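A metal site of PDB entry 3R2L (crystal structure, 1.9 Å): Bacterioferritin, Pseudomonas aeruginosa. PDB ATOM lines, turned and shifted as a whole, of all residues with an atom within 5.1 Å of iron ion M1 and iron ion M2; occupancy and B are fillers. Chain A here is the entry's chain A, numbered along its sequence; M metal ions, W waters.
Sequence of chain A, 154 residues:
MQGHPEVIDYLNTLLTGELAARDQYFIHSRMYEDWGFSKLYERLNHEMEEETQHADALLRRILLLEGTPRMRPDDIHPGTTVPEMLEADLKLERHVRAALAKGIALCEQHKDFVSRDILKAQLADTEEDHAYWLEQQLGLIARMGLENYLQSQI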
ATOM      1  N   GLU A  18     -34.813  24.668  -4.007  1.00  0.00           N
ATOM      2  CA  GLU A  18     -34.386  23.320  -3.538  1.00  0.00           C
ATOM      3  C   GLU A  18     -34.679  22.251  -4.614  1.00  0.00           C
ATOM      4  O   GLU A  18     -33.860  21.337  -4.830  1.00  0.00           O
ATOM      5  CB  GLU A  18     -35.089  22.923  -2.213  1.00  0.00           C
ATOM      6  CG  GLU A  18     -34.756  23.877  -1.099  1.00  0.00           C
ATOM      7  CD  GLU A  18     -33.263  23.925  -0.817  1.00  0.00           C
ATOM      8  OE1 GLU A  18     -32.677  22.868  -0.603  1.00  0.00           O
ATOM      9  OE2 GLU A  18     -32.666  25.004  -0.833  1.00  0.00           O
ATOM     10  N   TYR A  25     -27.857  18.405  -8.803  1.00  0.00           N
ATOM     11  CA  TYR A  25     -27.098  17.248  -8.282  1.00  0.00           C
ATOM     12  C   TYR A  25     -27.464  15.949  -9.007  1.00  0.00           C
ATOM     13  O   TYR A  25     -26.602  15.061  -9.171  1.00  0.00           O
ATOM     14  CB  TYR A  25     -27.419  17.088  -6.805  1.00  0.00           C
ATOM     15  CG  TYR A  25     -26.749  18.160  -5.943  1.00  0.00           C
ATOM     16  CD1 TYR A  25     -25.429  18.535  -6.181  1.00  0.00           C
ATOM     17  CD2 TYR A  25     -27.402  18.745  -4.881  1.00  0.00           C
ATOM     18  CE1 TYR A  25     -24.757  19.466  -5.346  1.00  0.00           C
ATOM     19  CE2 TYR A  25     -26.765  19.689  -4.066  1.00  0.00           C
ATOM     20  CZ  TYR A  25     -25.429  20.048  -4.305  1.00  0.00           C
ATOM     21  OH  TYR A  25     -24.767  20.976  -3.519  1.00  0.00           O
ATOM     22  N   GLU A  51     -31.342  17.235  -0.836  1.00  0.00           N
ATOM     23  CA  GLU A  51     -32.144  18.377  -1.327  1.00  0.00           C
ATOM     24  C   GLU A  51     -33.600  17.979  -1.495  1.00  0.00           C
ATOM     25  O   GLU A  51     -34.475  18.783  -1.364  1.00  0.00           O
ATOM     26  CB  GLU A  51     -31.635  18.920  -2.683  1.00  0.00           C
ATOM     27  CG  GLU A  51     -30.160  19.317  -2.711  1.00  0.00           C
ATOM     28  CD  GLU A  51     -29.788  20.488  -1.765  1.00  0.00           C
ATOM     29  OE1 GLU A  51     -30.615  20.979  -1.009  1.00  0.00           O
ATOM     30  OE2 GLU A  51     -28.644  20.905  -1.810  1.00  0.00           O
ATOM     31  N   HIS A  54     -34.977  18.492   1.757  1.00  0.00           N
ATOM     32  CA  HIS A  54     -35.135  19.927   2.068  1.00  0.00           C
ATOM     33  C   HIS A  54     -36.379  20.456   1.365  1.00  0.00           C
ATOM     34  O   HIS A  54     -37.186  21.167   1.939  1.00  0.00           O
ATOM     35  CB  HIS A  54     -33.938  20.735   1.582  1.00  0.00           C
ATOM     36  CG  HIS A  54     -32.719  20.582   2.422  1.00  0.00           C
ATOM     37  ND1 HIS A  54     -31.524  21.172   2.101  1.00  0.00           N
ATOM     38  CD2 HIS A  54     -32.507  19.920   3.587  1.00  0.00           C
ATOM     39  CE1 HIS A  54     -30.618  20.871   3.008  1.00  0.00           C
ATOM     40  NE2 HIS A  54     -31.191  20.120   3.933  1.00  0.00           N
ATOM     41  N   GLU A  93     -25.123  26.708  -3.960  1.00  0.00           N
ATOM     42  CA  GLU A  93     -25.248  26.610  -2.491  1.00  0.00           C
ATOM     43  C   GLU A  93     -25.064  27.989  -1.838  1.00  0.00           C
ATOM     44  O   GLU A  93     -25.708  28.268  -0.851  1.00  0.00           O
ATOM     45  CB  GLU A  93     -24.181  25.647  -1.919  1.00  0.00           C
ATOM     46  CG  GLU A  93     -24.420  24.185  -2.344  1.00  0.00           C
ATOM     47  CD  GLU A  93     -25.648  23.542  -1.638  1.00  0.00           C
ATOM     48  OE1 GLU A  93     -26.132  24.051  -0.598  1.00  0.00           O
ATOM     49  OE2 GLU A  93     -26.104  22.472  -2.112  1.00  0.00           O
ATOM     50  N   VAL A  96     -28.319  29.693  -2.207  1.00  0.00           N
ATOM     51  CA  VAL A  96     -29.272  29.122  -1.243  1.00  0.00           C
ATOM     52  C   VAL A  96     -29.001  29.642   0.168  1.00  0.00           C
ATOM     53  O   VAL A  96     -29.942  29.980   0.895  1.00  0.00           O
ATOM     54  CB  VAL A  96     -29.221  27.563  -1.245  1.00  0.00           C
ATOM     55  CG1 VAL A  96     -30.040  27.024  -0.063  1.00  0.00           C
ATOM     56  CG2 VAL A  96     -29.770  27.034  -2.565  1.00  0.00           C
ATOM     57  N   GLN A 122     -31.913  23.836   7.540  1.00  0.00           N
ATOM     58  CA  GLN A 122     -31.412  23.755   6.187  1.00  0.00           C
ATOM     59  C   GLN A 122     -30.204  24.625   5.973  1.00  0.00           C
ATOM     60  O   GLN A 122     -29.320  24.267   5.205  1.00  0.00           O
ATOM     61  CB  GLN A 122     -32.535  24.115   5.206  1.00  0.00           C
ATOM     62  CG  GLN A 122     -33.604  23.054   5.223  1.00  0.00           C
ATOM     63  CD  GLN A 122     -34.653  23.214   4.150  1.00  0.00           C
ATOM     64  OE1 GLN A 122     -35.732  22.597   4.234  1.00  0.00           O
ATOM     65  NE2 GLN A 122     -34.364  24.028   3.141  1.00  0.00           N
ATOM     66  N   THR A 126     -26.612  23.531   4.523  1.00  0.00           N
ATOM     67  CA  THR A 126     -26.013  24.240   3.382  1.00  0.00           C
ATOM     68  C   THR A 126     -24.574  24.707   3.678  1.00  0.00           C
ATOM     69  O   THR A 126     -23.635  24.449   2.913  1.00  0.00           O
ATOM     70  CB  THR A 126     -26.899  25.483   3.026  1.00  0.00           C
ATOM     71  OG1 THR A 126     -28.198  25.003   2.621  1.00  0.00           O
ATOM     72  CG2 THR A 126     -26.237  26.312   1.936  1.00  0.00           C
ATOM     73  N   HIS A 130     -22.990  20.872   2.636  1.00  0.00           N
ATOM     74  CA  HIS A 130     -22.943  21.019   1.162  1.00  0.00           C
ATOM     75  C   HIS A 130     -21.850  22.008   0.683  1.00  0.00           C
ATOM     76  O   HIS A 130     -20.942  21.631  -0.047  1.00  0.00           O
ATOM     77  CB  HIS A 130     -24.326  21.447   0.621  1.00  0.00           C
ATOM     78  CG  HIS A 130     -25.432  20.517   1.029  1.00  0.00           C
ATOM     79  ND1 HIS A 130     -26.746  20.693   0.634  1.00  0.00           N
ATOM     80  CD2 HIS A 130     -25.413  19.387   1.781  1.00  0.00           C
ATOM     81  CE1 HIS A 130     -27.481  19.710   1.132  1.00  0.00           C
ATOM     82  NE2 HIS A 130     -26.702  18.914   1.836  1.00  0.00           N
HETATM   83 FE    FE M   1     -30.965  22.516   0.394  1.00  0.00          FE
HETATM   84 FE    FE M   2     -27.650  22.226  -0.540  1.00  0.00          FE
HETATM   85  O   HOH W   1     -31.478  24.280   1.567  1.00  0.00           O
HETATM   86  O   HOH W   2     -29.006  23.051   0.756  1.00  0.00           O
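The side-chain carboxylate of Glu 93 lies close to the side-chain hydroxyl of Tyr 25 (2.5 Å).
The side-chain amide oxygen of Gln 122 sits close to the backbone carbonyl oxygen of His 54 (3.1 Å).
Three residues have an atom within 4 Å of iron ion M1: Glu 18, Glu 51 and His 54.
Within 4 Å of iron ion M2: Glu 51, Glu 93 and His 130.
The nearest printed residue that does not touch iron ion M2 is Thr 126 (4.2 Å).
Iron ion M1 is bound by OE1 of Glu 18 (2.0 Å), water W2 (2.1 Å), OE1 of Glu 51 (2.1 Å), water W1 (2.2 Å) and ND1 of His 54 (2.2 Å).
Iron ion M1 has five donor atoms within binding distance.
Water W2 binds iron ion M2 (2.0 Å).
The side-chain carboxylate (OE2) of Glu 51 binds iron ion M2, at 2.1 Å.
Iron ion M2 is bound by ND1 of His 130.
OE2 of Glu 93 is bound to iron ion M2, 2.2 Å away.
OE1 of Glu 93 is bound to iron ion M2 (2.4 Å).
Water W1 lies within hydrogen-bond range of the side-chain carboxylate of Glu 18 (2.8 Å) and the side-chain amide nitrogen of Gln 122 (3.3 Å).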
